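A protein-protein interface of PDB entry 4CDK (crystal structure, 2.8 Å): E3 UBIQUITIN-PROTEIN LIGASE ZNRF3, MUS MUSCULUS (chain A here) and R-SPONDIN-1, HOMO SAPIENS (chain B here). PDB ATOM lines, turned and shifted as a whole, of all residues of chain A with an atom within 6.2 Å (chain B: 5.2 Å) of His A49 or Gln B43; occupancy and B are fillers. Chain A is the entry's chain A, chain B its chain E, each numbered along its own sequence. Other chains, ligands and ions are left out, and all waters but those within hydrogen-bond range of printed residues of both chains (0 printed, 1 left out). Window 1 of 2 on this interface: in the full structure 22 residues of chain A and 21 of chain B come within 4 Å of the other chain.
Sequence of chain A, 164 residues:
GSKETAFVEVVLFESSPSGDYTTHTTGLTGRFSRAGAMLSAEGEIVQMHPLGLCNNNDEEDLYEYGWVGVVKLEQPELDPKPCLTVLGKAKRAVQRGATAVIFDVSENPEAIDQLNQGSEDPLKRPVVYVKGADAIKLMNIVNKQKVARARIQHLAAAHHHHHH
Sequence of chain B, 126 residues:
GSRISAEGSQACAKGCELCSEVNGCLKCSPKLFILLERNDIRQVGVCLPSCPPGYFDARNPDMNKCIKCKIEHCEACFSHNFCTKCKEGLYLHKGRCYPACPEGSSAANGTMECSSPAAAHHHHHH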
ATOM      1  N   GLN A  47     -25.620 -14.116   3.988  1.00  0.00           N
ATOM      2  CA  GLN A  47     -26.989 -13.871   3.542  1.00  0.00           C
ATOM      3  C   GLN A  47     -27.710 -15.203   3.364  1.00  0.00           C
ATOM      4  O   GLN A  47     -27.160 -16.144   2.788  1.00  0.00           O
ATOM      5  CB  GLN A  47     -27.010 -13.068   2.239  1.00  0.00           C
ATOM      6  CG  GLN A  47     -28.396 -12.613   1.806  1.00  0.00           C
ATOM      7  CD  GLN A  47     -28.774 -13.110   0.417  1.00  0.00           C
ATOM      8  OE1 GLN A  47     -27.988 -13.013  -0.524  1.00  0.00           O
ATOM      9  NE2 GLN A  47     -29.983 -13.641   0.286  1.00  0.00           N
ATOM     10  N   MET A  48     -28.938 -15.284   3.863  1.00  0.00           N
ATOM     11  CA  MET A  48     -29.711 -16.508   3.736  1.00  0.00           C
ATOM     12  C   MET A  48     -30.958 -16.265   2.910  1.00  0.00           C
ATOM     13  O   MET A  48     -31.712 -15.322   3.153  1.00  0.00           O
ATOM     14  CB  MET A  48     -30.098 -17.073   5.107  1.00  0.00           C
ATOM     15  CG  MET A  48     -28.925 -17.381   6.034  1.00  0.00           C
ATOM     16  SD  MET A  48     -27.879 -18.755   5.496  1.00  0.00           S
ATOM     17  CE  MET A  48     -29.087 -20.019   5.111  1.00  0.00           C
ATOM     18  N   HIS A  49     -31.150 -17.112   1.909  1.00  0.00           N
ATOM     19  CA  HIS A  49     -32.355 -17.100   1.104  1.00  0.00           C
ATOM     20  C   HIS A  49     -33.499 -17.588   1.987  1.00  0.00           C
ATOM     21  O   HIS A  49     -33.275 -18.419   2.860  1.00  0.00           O
ATOM     22  CB  HIS A  49     -32.168 -17.997  -0.123  1.00  0.00           C
ATOM     23  CG  HIS A  49     -33.277 -17.914  -1.121  1.00  0.00           C
ATOM     24  ND1 HIS A  49     -34.496 -18.536  -0.936  1.00  0.00           N
ATOM     25  CD2 HIS A  49     -33.346 -17.311  -2.332  1.00  0.00           C
ATOM     26  CE1 HIS A  49     -35.267 -18.303  -1.978  1.00  0.00           C
ATOM     27  NE2 HIS A  49     -34.594 -17.559  -2.842  1.00  0.00           N
ATOM     28  N   PRO A  50     -34.711 -17.044   1.799  1.00  0.00           N
ATOM     29  CA  PRO A  50     -35.883 -17.490   2.567  1.00  0.00           C
ATOM     30  C   PRO A  50     -36.004 -19.016   2.644  1.00  0.00           C
ATOM     31  O   PRO A  50     -36.242 -19.564   3.724  1.00  0.00           O
ATOM     32  CB  PRO A  50     -37.051 -16.888   1.790  1.00  0.00           C
ATOM     33  CG  PRO A  50     -36.489 -15.622   1.228  1.00  0.00           C
ATOM     34  CD  PRO A  50     -35.022 -15.879   0.951  1.00  0.00           C
ATOM     35  N   LEU A  51     -35.851 -19.683   1.505  1.00  0.00           N
ATOM     36  CA  LEU A  51     -35.866 -21.142   1.443  1.00  0.00           C
ATOM     37  C   LEU A  51     -34.612 -21.774   2.049  1.00  0.00           C
ATOM     38  O   LEU A  51     -34.554 -22.986   2.244  1.00  0.00           O
ATOM     39  CB  LEU A  51     -36.019 -21.603  -0.005  1.00  0.00           C
ATOM     40  CG  LEU A  51     -37.227 -21.049  -0.760  1.00  0.00           C
ATOM     41  CD1 LEU A  51     -37.167 -21.457  -2.222  1.00  0.00           C
ATOM     42  CD2 LEU A  51     -38.522 -21.517  -0.116  1.00  0.00           C
ATOM     43  N   GLY A  52     -33.611 -20.951   2.345  1.00  0.00           N
ATOM     44  CA  GLY A  52     -32.337 -21.437   2.852  1.00  0.00           C
ATOM     45  C   GLY A  52     -32.340 -21.987   4.265  1.00  0.00           C
ATOM     46  O   GLY A  52     -31.413 -22.690   4.661  1.00  0.00           O
ATOM     47  N   LEU A  53     -33.376 -21.671   5.031  1.00  0.00           N
ATOM     48  CA  LEU A  53     -33.474 -22.154   6.403  1.00  0.00           C
ATOM     49  C   LEU A  53     -34.550 -23.230   6.543  1.00  0.00           C
ATOM     50  O   LEU A  53     -34.984 -23.550   7.649  1.00  0.00           O
ATOM     51  CB  LEU A  53     -33.751 -20.992   7.361  1.00  0.00           C
ATOM     52  CG  LEU A  53     -32.631 -19.952   7.472  1.00  0.00           C
ATOM     53  CD1 LEU A  53     -33.169 -18.619   7.965  1.00  0.00           C
ATOM     54  CD2 LEU A  53     -31.522 -20.454   8.383  1.00  0.00           C
ATOM     55  N   CYS A  54     -34.976 -23.781   5.411  1.00  0.00           N
ATOM     56  CA  CYS A  54     -36.036 -24.785   5.385  1.00  0.00           C
ATOM     57  C   CYS A  54     -35.513 -26.203   5.599  1.00  0.00           C
ATOM     58  O   CYS A  54     -34.306 -26.428   5.684  1.00  0.00           O
ATOM     59  CB  CYS A  54     -36.795 -24.715   4.060  1.00  0.00           C
ATOM     60  SG  CYS A  54     -37.754 -23.203   3.827  1.00  0.00           S
ATOM     61  N   GLU A  60     -27.278 -27.810   3.801  1.00  0.00           N
ATOM     62  CA  GLU A  60     -26.760 -27.615   2.454  1.00  0.00           C
ATOM     63  C   GLU A  60     -25.241 -27.544   2.569  1.00  0.00           C
ATOM     64  O   GLU A  60     -24.505 -28.302   1.946  1.00  0.00           O
ATOM     65  CB  GLU A  60     -27.312 -26.325   1.841  1.00  0.00           C
ATOM     66  CG  GLU A  60     -27.133 -26.167   0.344  1.00  0.00           C
ATOM     67  CD  GLU A  60     -28.152 -26.997  -0.424  1.00  0.00           C
ATOM     68  OE1 GLU A  60     -28.963 -27.696   0.223  1.00  0.00           O
ATOM     69  OE2 GLU A  60     -28.161 -26.940  -1.671  1.00  0.00           O
ATOM     70  N   TYR A  63     -20.970 -23.934   8.062  1.00  0.00           N
ATOM     71  CA  TYR A  63     -20.186 -22.726   8.285  1.00  0.00           C
ATOM     72  C   TYR A  63     -19.450 -22.892   9.591  1.00  0.00           C
ATOM     73  O   TYR A  63     -19.877 -23.663  10.451  1.00  0.00           O
ATOM     74  CB  TYR A  63     -21.056 -21.475   8.397  1.00  0.00           C
ATOM     75  CG  TYR A  63     -22.265 -21.416   7.504  1.00  0.00           C
ATOM     76  CD1 TYR A  63     -22.161 -21.012   6.181  1.00  0.00           C
ATOM     77  CD2 TYR A  63     -23.527 -21.728   7.999  1.00  0.00           C
ATOM     78  CE1 TYR A  63     -23.277 -20.943   5.370  1.00  0.00           C
ATOM     79  CE2 TYR A  63     -24.646 -21.662   7.197  1.00  0.00           C
ATOM     80  CZ  TYR A  63     -24.517 -21.269   5.883  1.00  0.00           C
ATOM     81  OH  TYR A  63     -25.629 -21.201   5.076  1.00  0.00           O
ATOM     82  N   VAL A  70     -28.045 -12.928   7.662  1.00  0.00           N
ATOM     83  CA  VAL A  70     -28.777 -11.782   7.144  1.00  0.00           C
ATOM     84  C   VAL A  70     -29.859 -12.257   6.185  1.00  0.00           C
ATOM     85  O   VAL A  70     -29.581 -12.965   5.222  1.00  0.00           O
ATOM     86  CB  VAL A  70     -27.849 -10.790   6.432  1.00  0.00           C
ATOM     87  CG1 VAL A  70     -28.662  -9.730   5.726  1.00  0.00           C
ATOM     88  CG2 VAL A  70     -26.876 -10.161   7.429  1.00  0.00           C
ATOM     89  N   VAL A  71     -31.097 -11.867   6.458  1.00  0.00           N
ATOM     90  CA  VAL A  71     -32.231 -12.353   5.691  1.00  0.00           C
ATOM     91  C   VAL A  71     -33.098 -11.209   5.200  1.00  0.00           C
ATOM     92  O   VAL A  71     -33.608 -10.426   5.999  1.00  0.00           O
ATOM     93  CB  VAL A  71     -33.105 -13.307   6.529  1.00  0.00           C
ATOM     94  CG1 VAL A  71     -34.327 -13.744   5.738  1.00  0.00           C
ATOM     95  CG2 VAL A  71     -32.297 -14.510   6.990  1.00  0.00           C
ATOM     96  N   VAL B  22     -32.221  -9.080  -4.411  1.00  0.00           N
ATOM     97  CA  VAL B  22     -31.383  -9.671  -3.383  1.00  0.00           C
ATOM     98  C   VAL B  22     -31.430 -11.194  -3.438  1.00  0.00           C
ATOM     99  O   VAL B  22     -30.400 -11.851  -3.587  1.00  0.00           O
ATOM    100  CB  VAL B  22     -31.805  -9.194  -1.982  1.00  0.00           C
ATOM    101  CG1 VAL B  22     -31.006  -9.915  -0.903  1.00  0.00           C
ATOM    102  CG2 VAL B  22     -31.618  -7.693  -1.867  1.00  0.00           C
ATOM    103  N   ASN B  23     -32.633 -11.749  -3.340  1.00  0.00           N
ATOM    104  CA  ASN B  23     -32.798 -13.192  -3.196  1.00  0.00           C
ATOM    105  C   ASN B  23     -32.825 -13.976  -4.505  1.00  0.00           C
ATOM    106  O   ASN B  23     -32.943 -15.203  -4.494  1.00  0.00           O
ATOM    107  CB  ASN B  23     -34.070 -13.481  -2.398  1.00  0.00           C
ATOM    108  CG  ASN B  23     -33.941 -13.079  -0.943  1.00  0.00           C
ATOM    109  OD1 ASN B  23     -32.889 -13.261  -0.337  1.00  0.00           O
ATOM    110  ND2 ASN B  23     -35.007 -12.518  -0.380  1.00  0.00           N
ATOM    111  N   CYS B  25     -34.289 -15.744  -7.526  1.00  0.00           N
ATOM    112  CA  CYS B  25     -35.583 -16.338  -7.803  1.00  0.00           C
ATOM    113  C   CYS B  25     -36.234 -16.881  -6.535  1.00  0.00           C
ATOM    114  O   CYS B  25     -35.580 -17.505  -5.704  1.00  0.00           O
ATOM    115  CB  CYS B  25     -35.454 -17.451  -8.837  1.00  0.00           C
ATOM    116  SG  CYS B  25     -37.050 -17.961  -9.483  1.00  0.00           S
ATOM    117  N   LEU B  26     -37.532 -16.630  -6.399  1.00  0.00           N
ATOM    118  CA  LEU B  26     -38.289 -17.038  -5.222  1.00  0.00           C
ATOM    119  C   LEU B  26     -39.215 -18.214  -5.531  1.00  0.00           C
ATOM    120  O   LEU B  26     -39.495 -19.046  -4.665  1.00  0.00           O
ATOM    121  CB  LEU B  26     -39.099 -15.858  -4.684  1.00  0.00           C
ATOM    122  CG  LEU B  26     -38.281 -14.615  -4.332  1.00  0.00           C
ATOM    123  CD1 LEU B  26     -39.184 -13.406  -4.178  1.00  0.00           C
ATOM    124  CD2 LEU B  26     -37.470 -14.858  -3.068  1.00  0.00           C
ATOM    125  N   ILE B  34     -35.866 -25.284  -8.251  1.00  0.00           N
ATOM    126  CA  ILE B  34     -35.180 -24.130  -7.704  1.00  0.00           C
ATOM    127  C   ILE B  34     -33.921 -24.631  -7.005  1.00  0.00           C
ATOM    128  O   ILE B  34     -33.925 -25.683  -6.364  1.00  0.00           O
ATOM    129  CB  ILE B  34     -36.085 -23.308  -6.750  1.00  0.00           C
ATOM    130  CG1 ILE B  34     -35.449 -21.959  -6.422  1.00  0.00           C
ATOM    131  CG2 ILE B  34     -36.407 -24.070  -5.486  1.00  0.00           C
ATOM    132  CD1 ILE B  34     -36.464 -20.884  -6.111  1.00  0.00           C
ATOM    133  N   LEU B  36     -30.540 -23.177  -4.686  1.00  0.00           N
ATOM    134  CA  LEU B  36     -29.931 -22.058  -3.979  1.00  0.00           C
ATOM    135  C   LEU B  36     -28.431 -22.048  -4.197  1.00  0.00           C
ATOM    136  O   LEU B  36     -27.714 -22.938  -3.736  1.00  0.00           O
ATOM    137  CB  LEU B  36     -30.243 -22.111  -2.486  1.00  0.00           C
ATOM    138  CG  LEU B  36     -31.722 -22.016  -2.141  1.00  0.00           C
ATOM    139  CD1 LEU B  36     -31.879 -22.000  -0.640  1.00  0.00           C
ATOM    140  CD2 LEU B  36     -32.317 -20.772  -2.776  1.00  0.00           C
ATOM    141  N   GLU B  37     -27.971 -21.020  -4.901  1.00  0.00           N
ATOM    142  CA  GLU B  37     -26.561 -20.843  -5.205  1.00  0.00           C
ATOM    143  C   GLU B  37     -25.911 -19.853  -4.240  1.00  0.00           C
ATOM    144  O   GLU B  37     -26.326 -18.696  -4.142  1.00  0.00           O
ATOM    145  CB  GLU B  37     -26.398 -20.398  -6.664  1.00  0.00           C
ATOM    146  CG  GLU B  37     -24.981 -20.084  -7.098  1.00  0.00           C
ATOM    147  CD  GLU B  37     -23.973 -21.221  -6.975  1.00  0.00           C
ATOM    148  OE1 GLU B  37     -24.381 -22.385  -6.778  1.00  0.00           O
ATOM    149  OE2 GLU B  37     -22.752 -20.931  -7.036  1.00  0.00           O
ATOM    150  N   ARG B  38     -24.879 -20.308  -3.542  1.00  0.00           N
ATOM    151  CA  ARG B  38     -24.131 -19.426  -2.667  1.00  0.00           C
ATOM    152  C   ARG B  38     -22.930 -18.869  -3.414  1.00  0.00           C
ATOM    153  O   ARG B  38     -21.968 -19.583  -3.698  1.00  0.00           O
ATOM    154  CB  ARG B  38     -23.687 -20.154  -1.391  1.00  0.00           C
ATOM    155  CG  ARG B  38     -22.848 -19.294  -0.456  1.00  0.00           C
ATOM    156  CD  ARG B  38     -22.913 -19.779   0.985  1.00  0.00           C
ATOM    157  NE  ARG B  38     -24.285 -19.875   1.479  1.00  0.00           N
ATOM    158  CZ  ARG B  38     -25.019 -18.841   1.878  1.00  0.00           C
ATOM    159  NH1 ARG B  38     -24.536 -17.605   1.825  1.00  0.00           N
ATOM    160  NH2 ARG B  38     -26.253 -19.047   2.319  1.00  0.00           N
ATOM    161  N   ASN B  39     -23.019 -17.587  -3.745  1.00  0.00           N
ATOM    162  CA  ASN B  39     -21.920 -16.850  -4.346  1.00  0.00           C
ATOM    163  C   ASN B  39     -21.515 -15.741  -3.399  1.00  0.00           C
ATOM    164  O   ASN B  39     -22.290 -14.815  -3.156  1.00  0.00           O
ATOM    165  CB  ASN B  39     -22.300 -16.262  -5.707  1.00  0.00           C
ATOM    166  CG  ASN B  39     -22.939 -17.274  -6.624  1.00  0.00           C
ATOM    167  OD1 ASN B  39     -24.071 -17.089  -7.079  1.00  0.00           O
ATOM    168  ND2 ASN B  39     -22.209 -18.348  -6.918  1.00  0.00           N
ATOM    169  N   ILE B  41     -21.146 -13.786  -0.151  1.00  0.00           N
ATOM    170  CA  ILE B  41     -22.133 -13.677   0.912  1.00  0.00           C
ATOM    171  C   ILE B  41     -23.546 -14.041   0.442  1.00  0.00           C
ATOM    172  O   ILE B  41     -24.358 -14.547   1.219  1.00  0.00           O
ATOM    173  CB  ILE B  41     -22.143 -12.253   1.477  1.00  0.00           C
ATOM    174  CG1 ILE B  41     -20.711 -11.757   1.690  1.00  0.00           C
ATOM    175  CG2 ILE B  41     -22.942 -12.193   2.754  1.00  0.00           C
ATOM    176  CD1 ILE B  41     -20.584 -10.248   1.758  1.00  0.00           C
ATOM    177  N   ARG B  42     -23.815 -13.816  -0.839  1.00  0.00           N
ATOM    178  CA  ARG B  42     -25.164 -13.938  -1.387  1.00  0.00           C
ATOM    179  C   ARG B  42     -25.642 -15.379  -1.534  1.00  0.00           C
ATOM    180  O   ARG B  42     -24.871 -16.263  -1.908  1.00  0.00           O
ATOM    181  CB  ARG B  42     -25.237 -13.246  -2.750  1.00  0.00           C
ATOM    182  CG  ARG B  42     -24.979 -11.757  -2.718  1.00  0.00           C
ATOM    183  CD  ARG B  42     -24.800 -11.196  -4.123  1.00  0.00           C
ATOM    184  NE  ARG B  42     -25.922 -11.459  -5.024  1.00  0.00           N
ATOM    185  CZ  ARG B  42     -27.133 -10.922  -4.919  1.00  0.00           C
ATOM    186  NH1 ARG B  42     -27.414 -10.089  -3.925  1.00  0.00           N
ATOM    187  NH2 ARG B  42     -28.071 -11.232  -5.805  1.00  0.00           N
ATOM    188  N   GLN B  43     -26.924 -15.598  -1.255  1.00  0.00           N
ATOM    189  CA  GLN B  43     -27.580 -16.858  -1.592  1.00  0.00           C
ATOM    190  C   GLN B  43     -28.765 -16.588  -2.518  1.00  0.00           C
ATOM    191  O   GLN B  43     -29.764 -16.002  -2.100  1.00  0.00           O
ATOM    192  CB  GLN B  43     -28.048 -17.588  -0.331  1.00  0.00           C
ATOM    193  CG  GLN B  43     -28.315 -19.066  -0.549  1.00  0.00           C
ATOM    194  CD  GLN B  43     -28.852 -19.757   0.687  1.00  0.00           C
ATOM    195  OE1 GLN B  43     -29.595 -19.167   1.469  1.00  0.00           O
ATOM    196  NE2 GLN B  43     -28.486 -21.019   0.864  1.00  0.00           N
ATOM    197  N   VAL B  44     -28.668 -17.021  -3.770  1.00  0.00           N
ATOM    198  CA  VAL B  44     -29.676 -16.633  -4.755  1.00  0.00           C
ATOM    199  C   VAL B  44     -30.389 -17.836  -5.367  1.00  0.00           C
ATOM    200  O   VAL B  44     -29.781 -18.881  -5.627  1.00  0.00           O
ATOM    201  CB  VAL B  44     -29.064 -15.772  -5.891  1.00  0.00           C
ATOM    202  CG1 VAL B  44     -28.317 -14.583  -5.308  1.00  0.00           C
ATOM    203  CG2 VAL B  44     -28.139 -16.593  -6.758  1.00  0.00           C
ATOM    204  N   GLY B  45     -31.694 -17.689  -5.568  1.00  0.00           N
ATOM    205  CA  GLY B  45     -32.474 -18.726  -6.209  1.00  0.00           C
ATOM    206  C   GLY B  45     -32.227 -18.743  -7.705  1.00  0.00           C
ATOM    207  O   GLY B  45     -32.083 -17.694  -8.334  1.00  0.00           O
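Of chain B, only Asn B23, Cys B25, Leu B26, Leu B36, Gln B43 and Gly B45 come within 4 Å of His A49. Gln B43 touches just these residues of chain A: Gln A47, Met A48, His A49 and Gly A52. Printed residues of chain B within 4 Å of Pro A50: Asn B23 (3.5 Å). Printed residues of chain A within 4 Å of Asn B23: Gln A47, His A49 and Pro A50. Printed residues of chain A within 4 Å of Gly B45: His A49 (3.7 Å). Val A70 touches none of the printed residues of chain B. Leu A53 touches none of the printed residues of chain B. The nearest residue of chain B that does not touch His A49 is Val B44 (4.3 Å). The nearest residue of chain A that does not touch Gln B43 is Tyr A63 (5.1 Å).
The side-chain sulfur (SD) of Met A48 lies within hydrogen-bond range of the side-chain hydroxyl (OH) of Tyr A63 (3.3 Å). O of Val A70 lies within hydrogen-bond range of N of Met A48 (2.8 Å). A ring nitrogen (ND1) of His A49 is in hydrogen-bond range of the backbone NH of Leu A51, at 3.0 Å. NH2 of Arg B42 is in hydrogen-bond range of O of Val B22, 3.3 Å away. NH1 of Arg B38 lies within hydrogen-bond range of O of Ile B41, at 3.1 Å. The guanidinium group (NH2) of Arg B38 lies close to the side-chain amide nitrogen (NE2) of Gln B43 (3.3 Å).
The side-chain amide nitrogen (NE2) of Gln A47 lies within hydrogen-bond range of the side-chain amide oxygen (OD1) of Asn B23 (3.0 Å). The backbone carbonyl oxygen (O) of Gln A47 sits at hydrogen-bond distance from the guanidinium group (NH2) of Arg B38 (3.1 Å). N of Gln A47 lies within hydrogen-bond range of O of Ile B41, 3.1 Å away. The backbone NH (N) of Gln B43 sits at hydrogen-bond distance from the side-chain amide oxygen (OE1) of Gln A47, at 2.9 Å. NH2 of Arg B38 sits at hydrogen-bond distance from SD of Met A48, at 3.6 Å. A ring nitrogen (NE2) of His A49 lies close to the backbone carbonyl oxygen of Asn B23 (3.3 Å). NE2 of His A49 sits at hydrogen-bond distance from O of Cys B25 (3.0 Å). OE1 of Gln B43 lies within hydrogen-bond range of N of His A49.
CA of Arg B42 touches OE1 of Gln A47, at 3.1 Å. OE1 of Gln B43 touches CA of Met A48, 3.5 Å away. NE2 of His A49 touches CD2 of Leu B26, 3.95 Å away. CD2 of Leu B36 touches CG of His A49 (3.4 Å). CD2 of His A49 touches N of Gly B45 (3.7 Å). CG of Asn B23 touches CD of Pro A50, 3.5 Å away. Leu A51 touches Ile B34 (CD1 to CD1, 3.99 Å). Leu A51 touches Leu B36. Gln B43 touches Gly A52 (OE1 to CA, 3.8 Å). OH of Tyr A63 touches NH2 of Arg B38, 3.6 Å away.
Of the 12 printed residues of chain A, 7 touch a printed residue of chain B. Of the 14 printed residues of chain B, 10 touch a printed residue of chain A. Printed residues of chain B that touch a printed residue of chain A: Asn B23, Cys B25, Leu B26, Ile B34, Leu B36, Arg B38, Ile B41, Arg B42, Gln B43 and Gly B45. Hydrophobic or aromatic side chains of chain B within 4 Å of the printed part of chain A: Leu B26, Ile B34, Leu B36 and Ile B41.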
